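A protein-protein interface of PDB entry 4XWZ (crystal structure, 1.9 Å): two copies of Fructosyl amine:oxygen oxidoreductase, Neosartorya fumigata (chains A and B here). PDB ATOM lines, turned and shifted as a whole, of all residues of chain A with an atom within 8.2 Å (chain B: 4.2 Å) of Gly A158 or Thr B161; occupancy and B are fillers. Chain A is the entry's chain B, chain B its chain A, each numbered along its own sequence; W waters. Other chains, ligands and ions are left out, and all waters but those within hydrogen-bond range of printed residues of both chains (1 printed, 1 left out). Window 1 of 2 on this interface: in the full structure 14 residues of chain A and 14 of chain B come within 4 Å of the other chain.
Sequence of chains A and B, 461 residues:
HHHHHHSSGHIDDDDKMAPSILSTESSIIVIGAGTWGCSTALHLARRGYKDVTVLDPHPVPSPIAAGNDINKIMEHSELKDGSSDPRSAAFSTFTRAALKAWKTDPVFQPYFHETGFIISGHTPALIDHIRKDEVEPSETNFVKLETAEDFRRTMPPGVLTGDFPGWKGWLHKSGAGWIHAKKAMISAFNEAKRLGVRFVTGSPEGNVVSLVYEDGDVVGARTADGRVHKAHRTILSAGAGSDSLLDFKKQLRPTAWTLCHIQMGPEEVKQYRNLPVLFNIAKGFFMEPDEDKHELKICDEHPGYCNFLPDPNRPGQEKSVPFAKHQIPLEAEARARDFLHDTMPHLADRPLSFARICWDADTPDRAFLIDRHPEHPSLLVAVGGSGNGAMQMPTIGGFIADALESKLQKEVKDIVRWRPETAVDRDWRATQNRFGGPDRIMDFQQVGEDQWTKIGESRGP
Of the printed residues of chain B, Pro A157 touches Thr B161, Pro B345 and His B346. Of chain B, only Thr B161 (3.6 Å) comes within 4 Å of Gly A158. Of the printed residues of chain B, Thr A161 touches Gly B158. Gly A162 touches none of the printed residues of chain B. Printed residues of chain B within 4 Å of Gln A271: His B346 (3.6 Å). Of chain A, only Pro A157 (3.9 Å) and Gly A158 (3.6 Å) come within 4 Å of Thr B161. Of the printed residues of chain A, His B346 touches Pro A157 and Gln A271.
Arg A152 touches its own counterpart, Arg B152. Gly A158 touches Thr B161, and with the chains exchanged Thr A161 touches Gly B158. Positions printed for both chains: 152, 158, 159, 160, 161, 162, 343, 344 and 346.
Of the 18 printed residues of chain A, 5 touch a printed residue of chain B. Hydrophobic or aromatic side chains of chain A within 4 Å of the printed part of chain B: Pro A157. Of the 10 printed residues of chain B, 5 touch a printed residue of chain A. Printed residues of chain B that touch a printed residue of chain A: Arg B152, Gly B158, Thr B161, Pro B345 and His B346. Hydrophobic or aromatic side chains of chain B within 4 Å of the printed part of chain A: Pro B345 and His B346. Among the printed residues, no Asp or Glu carboxylate lies within 4 Å of a Lys or Arg side-chain nitrogen of the other chain.
Water W1 lies within hydrogen-bond range of the guanidinium group of Arg A152 (3.0 Å) and the guanidinium group of Arg B152 (3.4 Å).
NH1 of Arg A152 lies within hydrogen-bond range of O of Gly A162 (2.9 Å). O of Gly B158 sits at hydrogen-bond distance from NE2 of His B346 (3.5 Å). NH1 of Arg B152 sits at hydrogen-bond distance from O of Gly B162. OG1 of Thr A161 is in hydrogen-bond range of ND1 of His A346 (2.7 Å). N of Thr B161 sits at hydrogen-bond distance from O of Thr B343 (3.0 Å). O of Pro A157 is in hydrogen-bond range of NE2 of Gln A271.
The guanidinium group (NH2) of Arg B152 sits close to the guanidinium group (NH2) of Arg A152.
Among the printed residues, pairs that only touch across the chains: Pro A157 with His B346 (3.3 Å), Gln A271 with His B346 (3.6 Å), Gly A158 with Thr B161 (3.6 Å), Thr A161 with Gly B158 (3.7 Å), Pro A157 with Pro B345 (3.9 Å) and Pro A157 with Thr B161 (3.9 Å).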
ATOM      1  N   ARG A 152      13.204   0.356   7.801  1.00  0.00           N
ATOM      2  CA  ARG A 152      14.022   1.100   6.844  1.00  0.00           C
ATOM      3  C   ARG A 152      14.064   2.593   7.176  1.00  0.00           C
ATOM      4  O   ARG A 152      15.100   3.238   7.032  1.00  0.00           O
ATOM      5  CB  ARG A 152      13.512   0.881   5.420  1.00  0.00           C
ATOM      6  CG  ARG A 152      13.825  -0.511   4.881  1.00  0.00           C
ATOM      7  CD  ARG A 152      13.585  -0.616   3.382  1.00  0.00           C
ATOM      8  NE  ARG A 152      12.234  -0.219   3.015  1.00  0.00           N
ATOM      9  CZ  ARG A 152      11.223  -1.064   2.854  1.00  0.00           C
ATOM     10  NH1 ARG A 152      11.400  -2.362   3.054  1.00  0.00           N
ATOM     11  NH2 ARG A 152      10.003  -0.595   2.637  1.00  0.00           N
ATOM     12  N   ARG A 153      12.996   3.087   7.791  1.00  0.00           N
ATOM     13  CA  ARG A 153      12.896   4.504   8.112  1.00  0.00           C
ATOM     14  C   ARG A 153      13.717   4.908   9.332  1.00  0.00           C
ATOM     15  O   ARG A 153      13.812   6.093   9.642  1.00  0.00           O
ATOM     16  CB  ARG A 153      11.436   4.896   8.331  1.00  0.00           C
ATOM     17  CG  ARG A 153      10.635   5.001   7.049  1.00  0.00           C
ATOM     18  CD  ARG A 153       9.395   5.856   7.240  1.00  0.00           C
ATOM     19  NE  ARG A 153       8.959   6.443   5.981  1.00  0.00           N
ATOM     20  CZ  ARG A 153       7.871   6.068   5.321  1.00  0.00           C
ATOM     21  NH1 ARG A 153       7.018   5.223   5.881  1.00  0.00           N
ATOM     22  NH2 ARG A 153       7.562   6.651   4.174  1.00  0.00           N
ATOM     23  N   MET A 155      16.837   4.615   9.489  1.00  0.00           N
ATOM     24  CA  MET A 155      18.140   5.050   8.982  1.00  0.00           C
ATOM     25  C   MET A 155      17.989   5.803   7.662  1.00  0.00           C
ATOM     26  O   MET A 155      16.917   5.790   7.057  1.00  0.00           O
ATOM     27  CB  MET A 155      19.058   3.842   8.789  1.00  0.00           C
ATOM     28  CG  MET A 155      19.331   3.063  10.068  1.00  0.00           C
ATOM     29  SD  MET A 155      20.499   1.716   9.823  1.00  0.00           S
ATOM     30  CE  MET A 155      20.198   0.755  11.312  1.00  0.00           C
ATOM     31  N   PRO A 156      19.030   6.552   7.266  1.00  0.00           N
ATOM     32  CA  PRO A 156      18.936   7.378   6.064  1.00  0.00           C
ATOM     33  C   PRO A 156      18.676   6.527   4.825  1.00  0.00           C
ATOM     34  O   PRO A 156      19.029   5.348   4.807  1.00  0.00           O
ATOM     35  CB  PRO A 156      20.315   8.037   5.982  1.00  0.00           C
ATOM     36  CG  PRO A 156      20.816   8.039   7.389  1.00  0.00           C
ATOM     37  CD  PRO A 156      20.290   6.772   7.993  1.00  0.00           C
ATOM     38  N   PRO A 157      18.036   7.111   3.802  1.00  0.00           N
ATOM     39  CA  PRO A 157      17.694   6.340   2.607  1.00  0.00           C
ATOM     40  C   PRO A 157      18.928   5.757   1.929  1.00  0.00           C
ATOM     41  O   PRO A 157      19.989   6.386   1.927  1.00  0.00           O
ATOM     42  CB  PRO A 157      17.003   7.368   1.694  1.00  0.00           C
ATOM     43  CG  PRO A 157      17.291   8.712   2.290  1.00  0.00           C
ATOM     44  CD  PRO A 157      17.513   8.488   3.753  1.00  0.00           C
ATOM     45  N   GLY A 158      18.844   4.484   1.556  1.00  0.00           N
ATOM     46  CA  GLY A 158      19.936   3.817   0.866  1.00  0.00           C
ATOM     47  C   GLY A 158      20.785   2.974   1.797  1.00  0.00           C
ATOM     48  O   GLY A 158      21.613   2.185   1.345  1.00  0.00           O
ATOM     49  N   VAL A 159      20.509   3.061   3.095  1.00  0.00           N
ATOM     50  CA  VAL A 159      21.204   2.228   4.066  1.00  0.00           C
ATOM     51  C   VAL A 159      20.508   0.885   4.247  1.00  0.00           C
ATOM     52  O   VAL A 159      21.071  -0.161   3.922  1.00  0.00           O
ATOM     53  CB  VAL A 159      21.327   2.939   5.420  1.00  0.00           C
ATOM     54  CG1 VAL A 159      21.942   2.010   6.456  1.00  0.00           C
ATOM     55  CG2 VAL A 159      22.152   4.209   5.267  1.00  0.00           C
ATOM     56  N   LEU A 160      19.274   0.918   4.741  1.00  0.00           N
ATOM     57  CA  LEU A 160      18.453  -0.283   4.834  1.00  0.00           C
ATOM     58  C   LEU A 160      17.547  -0.435   3.611  1.00  0.00           C
ATOM     59  O   LEU A 160      16.758   0.456   3.289  1.00  0.00           O
ATOM     60  CB  LEU A 160      17.614  -0.258   6.113  1.00  0.00           C
ATOM     61  CG  LEU A 160      18.410  -0.120   7.411  1.00  0.00           C
ATOM     62  CD1 LEU A 160      17.490  -0.031   8.620  1.00  0.00           C
ATOM     63  CD2 LEU A 160      19.398  -1.270   7.572  1.00  0.00           C
ATOM     64  N   THR A 161      17.720  -1.542   2.899  1.00  0.00           N
ATOM     65  CA  THR A 161      17.074  -1.752   1.610  1.00  0.00           C
ATOM     66  C   THR A 161      16.333  -3.082   1.595  1.00  0.00           C
ATOM     67  O   THR A 161      15.718  -3.440   0.594  1.00  0.00           O
ATOM     68  CB  THR A 161      18.100  -1.765   0.462  1.00  0.00           C
ATOM     69  OG1 THR A 161      19.083  -2.784   0.698  1.00  0.00           O
ATOM     70  CG2 THR A 161      18.786  -0.415   0.340  1.00  0.00           C
ATOM     71  N   GLY A 162      16.330  -3.776   2.730  1.00  0.00           N
ATOM     72  CA  GLY A 162      15.840  -5.146   2.787  1.00  0.00           C
ATOM     73  C   GLY A 162      14.339  -5.257   2.987  1.00  0.00           C
ATOM     74  O   GLY A 162      13.652  -4.259   3.221  1.00  0.00           O
ATOM     75  N   MET A 264      33.561  -0.212   2.868  1.00  0.00           N
ATOM     76  CA  MET A 264      32.639   0.647   2.138  1.00  0.00           C
ATOM     77  C   MET A 264      33.413   1.614   1.246  1.00  0.00           C
ATOM     78  O   MET A 264      34.587   1.882   1.489  1.00  0.00           O
ATOM     79  CB  MET A 264      31.755   1.421   3.113  1.00  0.00           C
ATOM     80  CG  MET A 264      31.041   0.539   4.124  1.00  0.00           C
ATOM     81  SD  MET A 264      29.954  -0.669   3.341  1.00  0.00           S
ATOM     82  CE  MET A 264      28.635   0.407   2.780  1.00  0.00           C
ATOM     83  N   GLU A 268      29.629   5.949  -1.036  1.00  0.00           N
ATOM     84  CA  GLU A 268      28.495   5.249  -0.445  1.00  0.00           C
ATOM     85  C   GLU A 268      28.543   5.336   1.081  1.00  0.00           C
ATOM     86  O   GLU A 268      27.505   5.458   1.733  1.00  0.00           O
ATOM     87  CB  GLU A 268      28.452   3.788  -0.901  1.00  0.00           C
ATOM     88  CG  GLU A 268      29.664   2.979  -0.498  1.00  0.00           C
ATOM     89  CD  GLU A 268      29.482   1.491  -0.724  1.00  0.00           C
ATOM     90  OE1 GLU A 268      28.404   1.072  -1.202  1.00  0.00           O
ATOM     91  OE2 GLU A 268      30.437   0.743  -0.447  1.00  0.00           O
ATOM     92  N   GLN A 271      26.389   8.057   3.483  1.00  0.00           N
ATOM     93  CA  GLN A 271      25.021   7.880   3.964  1.00  0.00           C
ATOM     94  C   GLN A 271      25.004   7.171   5.317  1.00  0.00           C
ATOM     95  O   GLN A 271      23.993   7.199   6.022  1.00  0.00           O
ATOM     96  CB  GLN A 271      24.199   7.069   2.959  1.00  0.00           C
ATOM     97  CG  GLN A 271      23.537   7.888   1.860  1.00  0.00           C
ATOM     98  CD  GLN A 271      22.762   9.083   2.387  1.00  0.00           C
ATOM     99  OE1 GLN A 271      23.311  10.176   2.491  1.00  0.00           O
ATOM    100  NE2 GLN A 271      21.445   8.931   2.499  1.00  0.00           N
ATOM    101  N   TYR A 272      26.046   6.387   5.587  1.00  0.00           N
ATOM    102  CA  TYR A 272      26.009   5.419   6.677  1.00  0.00           C
ATOM    103  C   TYR A 272      26.484   6.041   7.988  1.00  0.00           C
ATOM    104  O   TYR A 272      27.430   5.558   8.601  1.00  0.00           O
ATOM    105  CB  TYR A 272      26.884   4.208   6.345  1.00  0.00           C
ATOM    106  CG  TYR A 272      26.304   3.302   5.284  1.00  0.00           C
ATOM    107  CD1 TYR A 272      26.389   3.638   3.944  1.00  0.00           C
ATOM    108  CD2 TYR A 272      25.734   2.081   5.620  1.00  0.00           C
ATOM    109  CE1 TYR A 272      25.947   2.777   2.964  1.00  0.00           C
ATOM    110  CE2 TYR A 272      25.298   1.205   4.645  1.00  0.00           C
ATOM    111  CZ  TYR A 272      25.366   1.580   3.322  1.00  0.00           C
ATOM    112  OH  TYR A 272      24.927   0.731   2.338  1.00  0.00           O
ATOM    113  N   THR A 343      18.415  -7.217   5.490  1.00  0.00           N
ATOM    114  CA  THR A 343      18.516  -5.844   5.973  1.00  0.00           C
ATOM    115  C   THR A 343      19.127  -4.923   4.918  1.00  0.00           C
ATOM    116  O   THR A 343      18.576  -3.863   4.609  1.00  0.00           O
ATOM    117  CB  THR A 343      19.376  -5.777   7.248  1.00  0.00           C
ATOM    118  OG1 THR A 343      20.685  -6.299   6.975  1.00  0.00           O
ATOM    119  CG2 THR A 343      18.728  -6.584   8.369  1.00  0.00           C
ATOM    120  N   MET A 344      20.236  -5.363   4.332  1.00  0.00           N
ATOM    121  CA  MET A 344      20.979  -4.566   3.361  1.00  0.00           C
ATOM    122  C   MET A 344      21.430  -5.449   2.199  1.00  0.00           C
ATOM    123  O   MET A 344      22.623  -5.679   2.006  1.00  0.00           O
ATOM    124  CB  MET A 344      22.188  -3.901   4.030  1.00  0.00           C
ATOM    125  CG  MET A 344      21.814  -2.942   5.154  1.00  0.00           C
ATOM    126  SD  MET A 344      23.222  -2.078   5.886  1.00  0.00           S
ATOM    127  CE  MET A 344      24.042  -3.445   6.706  1.00  0.00           C
ATOM    128  N   HIS A 346      21.882  -5.162  -0.767  1.00  0.00           N
ATOM    129  CA  HIS A 346      22.846  -4.600  -1.712  1.00  0.00           C
ATOM    130  C   HIS A 346      24.290  -4.844  -1.271  1.00  0.00           C
ATOM    131  O   HIS A 346      25.209  -4.790  -2.090  1.00  0.00           O
ATOM    132  CB  HIS A 346      22.595  -3.106  -1.925  1.00  0.00           C
ATOM    133  CG  HIS A 346      22.665  -2.293  -0.670  1.00  0.00           C
ATOM    134  ND1 HIS A 346      21.728  -2.393   0.335  1.00  0.00           N
ATOM    135  CD2 HIS A 346      23.560  -1.367  -0.257  1.00  0.00           C
ATOM    136  CE1 HIS A 346      22.011  -1.521   1.286  1.00  0.00           C
ATOM    137  NE2 HIS A 346      23.127  -0.897   0.960  1.00  0.00           N
ATOM    138  N   LEU A 347      24.467  -5.288  -0.030  1.00  0.00           N
ATOM    139  CA  LEU A 347      25.801  -5.554   0.503  1.00  0.00           C
ATOM    140  C   LEU A 347      26.079  -7.050   0.674  1.00  0.00           C
ATOM    141  O   LEU A 347      27.190  -7.437   1.034  1.00  0.00           O
ATOM    142  CB  LEU A 347      25.989  -4.851   1.851  1.00  0.00           C
ATOM    143  CG  LEU A 347      25.902  -3.322   1.876  1.00  0.00           C
ATOM    144  CD1 LEU A 347      26.182  -2.811   3.280  1.00  0.00           C
ATOM    145  CD2 LEU A 347      26.847  -2.676   0.871  1.00  0.00           C
ATOM    146  N   ARG B 152      10.289   0.527  -6.485  1.00  0.00           N
ATOM    147  CA  ARG B 152      11.632   0.228  -6.002  1.00  0.00           C
ATOM    148  C   ARG B 152      12.085  -1.160  -6.448  1.00  0.00           C
ATOM    149  O   ARG B 152      13.260  -1.358  -6.759  1.00  0.00           O
ATOM    150  CB  ARG B 152      11.709   0.354  -4.480  1.00  0.00           C
ATOM    151  CG  ARG B 152      11.617   1.795  -3.988  1.00  0.00           C
ATOM    152  CD  ARG B 152      11.996   1.926  -2.524  1.00  0.00           C
ATOM    153  NE  ARG B 152      11.149   1.107  -1.664  1.00  0.00           N
ATOM    154  CZ  ARG B 152      10.097   1.561  -0.992  1.00  0.00           C
ATOM    155  NH1 ARG B 152       9.722   2.827  -1.114  1.00  0.00           N
ATOM    156  NH2 ARG B 152       9.366   0.726  -0.268  1.00  0.00           N
ATOM    157  N   GLY B 158      19.118  -0.643  -3.299  1.00  0.00           N
ATOM    158  CA  GLY B 158      20.054   0.446  -3.092  1.00  0.00           C
ATOM    159  C   GLY B 158      19.947   1.514  -4.162  1.00  0.00           C
ATOM    160  O   GLY B 158      20.482   2.605  -4.001  1.00  0.00           O
ATOM    161  N   VAL B 159      19.239   1.216  -5.247  1.00  0.00           N
ATOM    162  CA  VAL B 159      19.141   2.163  -6.356  1.00  0.00           C
ATOM    163  C   VAL B 159      17.974   3.130  -6.150  1.00  0.00           C
ATOM    164  O   VAL B 159      18.182   4.314  -5.882  1.00  0.00           O
ATOM    165  CB  VAL B 159      19.001   1.447  -7.713  1.00  0.00           C
ATOM    166  CG1 VAL B 159      18.787   2.463  -8.825  1.00  0.00           C
ATOM    167  CG2 VAL B 159      20.237   0.601  -7.996  1.00  0.00           C
ATOM    168  N   LEU B 160      16.760   2.596  -6.127  1.00  0.00           N
ATOM    169  CA  LEU B 160      15.591   3.396  -5.795  1.00  0.00           C
ATOM    170  C   LEU B 160      15.253   3.260  -4.315  1.00  0.00           C
ATOM    171  O   LEU B 160      14.973   2.163  -3.825  1.00  0.00           O
ATOM    172  CB  LEU B 160      14.393   2.976  -6.645  1.00  0.00           C
ATOM    173  CG  LEU B 160      14.604   3.027  -8.157  1.00  0.00           C
ATOM    174  CD1 LEU B 160      13.376   2.489  -8.871  1.00  0.00           C
ATOM    175  CD2 LEU B 160      14.921   4.443  -8.617  1.00  0.00           C
ATOM    176  N   THR B 161      15.225   4.393  -3.622  1.00  0.00           N
ATOM    177  CA  THR B 161      15.105   4.398  -2.177  1.00  0.00           C
ATOM    178  C   THR B 161      13.970   5.314  -1.732  1.00  0.00           C
ATOM    179  O   THR B 161      13.732   5.476  -0.541  1.00  0.00           O
ATOM    180  CB  THR B 161      16.414   4.868  -1.521  1.00  0.00           C
ATOM    181  OG1 THR B 161      16.758   6.167  -2.021  1.00  0.00           O
ATOM    182  CG2 THR B 161      17.543   3.895  -1.830  1.00  0.00           C
ATOM    183  N   GLY B 162      13.308   5.953  -2.690  1.00  0.00           N
ATOM    184  CA  GLY B 162      12.374   7.029  -2.390  1.00  0.00           C
ATOM    185  C   GLY B 162      10.996   6.530  -1.994  1.00  0.00           C
ATOM    186  O   GLY B 162      10.714   5.330  -2.065  1.00  0.00           O
ATOM    187  N   THR B 343      12.647   9.772  -5.650  1.00  0.00           N
ATOM    188  CA  THR B 343      13.034   8.494  -6.250  1.00  0.00           C
ATOM    189  C   THR B 343      14.305   7.934  -5.613  1.00  0.00           C
ATOM    190  O   THR B 343      14.387   6.737  -5.307  1.00  0.00           O
ATOM    191  CB  THR B 343      13.294   8.643  -7.762  1.00  0.00           C
ATOM    192  OG1 THR B 343      14.314   9.627  -7.986  1.00  0.00           O
ATOM    193  CG2 THR B 343      12.019   9.052  -8.487  1.00  0.00           C
ATOM    194  N   MET B 344      15.326   8.785  -5.535  1.00  0.00           N
ATOM    195  CA  MET B 344      16.633   8.415  -5.007  1.00  0.00           C
ATOM    196  C   MET B 344      17.150   9.509  -4.075  1.00  0.00           C
ATOM    197  O   MET B 344      18.126  10.186  -4.386  1.00  0.00           O
ATOM    198  CB  MET B 344      17.626   8.210  -6.154  1.00  0.00           C
ATOM    199  CG  MET B 344      17.245   7.076  -7.092  1.00  0.00           C
ATOM    200  SD  MET B 344      18.473   6.770  -8.379  1.00  0.00           S
ATOM    201  CE  MET B 344      18.302   8.268  -9.345  1.00  0.00           C
ATOM    202  N   PRO B 345      16.485   9.691  -2.927  1.00  0.00           N
ATOM    203  CA  PRO B 345      16.764  10.831  -2.061  1.00  0.00           C
ATOM    204  C   PRO B 345      18.179  10.810  -1.493  1.00  0.00           C
ATOM    205  O   PRO B 345      18.715  11.858  -1.142  1.00  0.00           O
ATOM    206  CB  PRO B 345      15.725  10.694  -0.933  1.00  0.00           C
ATOM    207  CG  PRO B 345      15.135   9.328  -1.081  1.00  0.00           C
ATOM    208  CD  PRO B 345      15.257   8.989  -2.532  1.00  0.00           C
ATOM    209  N   HIS B 346      18.814   9.643  -1.487  1.00  0.00           N
ATOM    210  CA  HIS B 346      20.197   9.550  -1.036  1.00  0.00           C
ATOM    211  C   HIS B 346      21.166  10.260  -1.985  1.00  0.00           C
ATOM    212  O   HIS B 346      22.278  10.605  -1.582  1.00  0.00           O
ATOM    213  CB  HIS B 346      20.615   8.085  -0.855  1.00  0.00           C
ATOM    214  CG  HIS B 346      20.521   7.270  -2.107  1.00  0.00           C
ATOM    215  ND1 HIS B 346      19.316   6.926  -2.681  1.00  0.00           N
ATOM    216  CD2 HIS B 346      21.481   6.732  -2.895  1.00  0.00           C
ATOM    217  CE1 HIS B 346      19.538   6.211  -3.768  1.00  0.00           C
ATOM    218  NE2 HIS B 346      20.843   6.061  -3.909  1.00  0.00           N
HETATM  219  O   HOH W   1       9.907   2.403   2.585  1.00  0.00           O
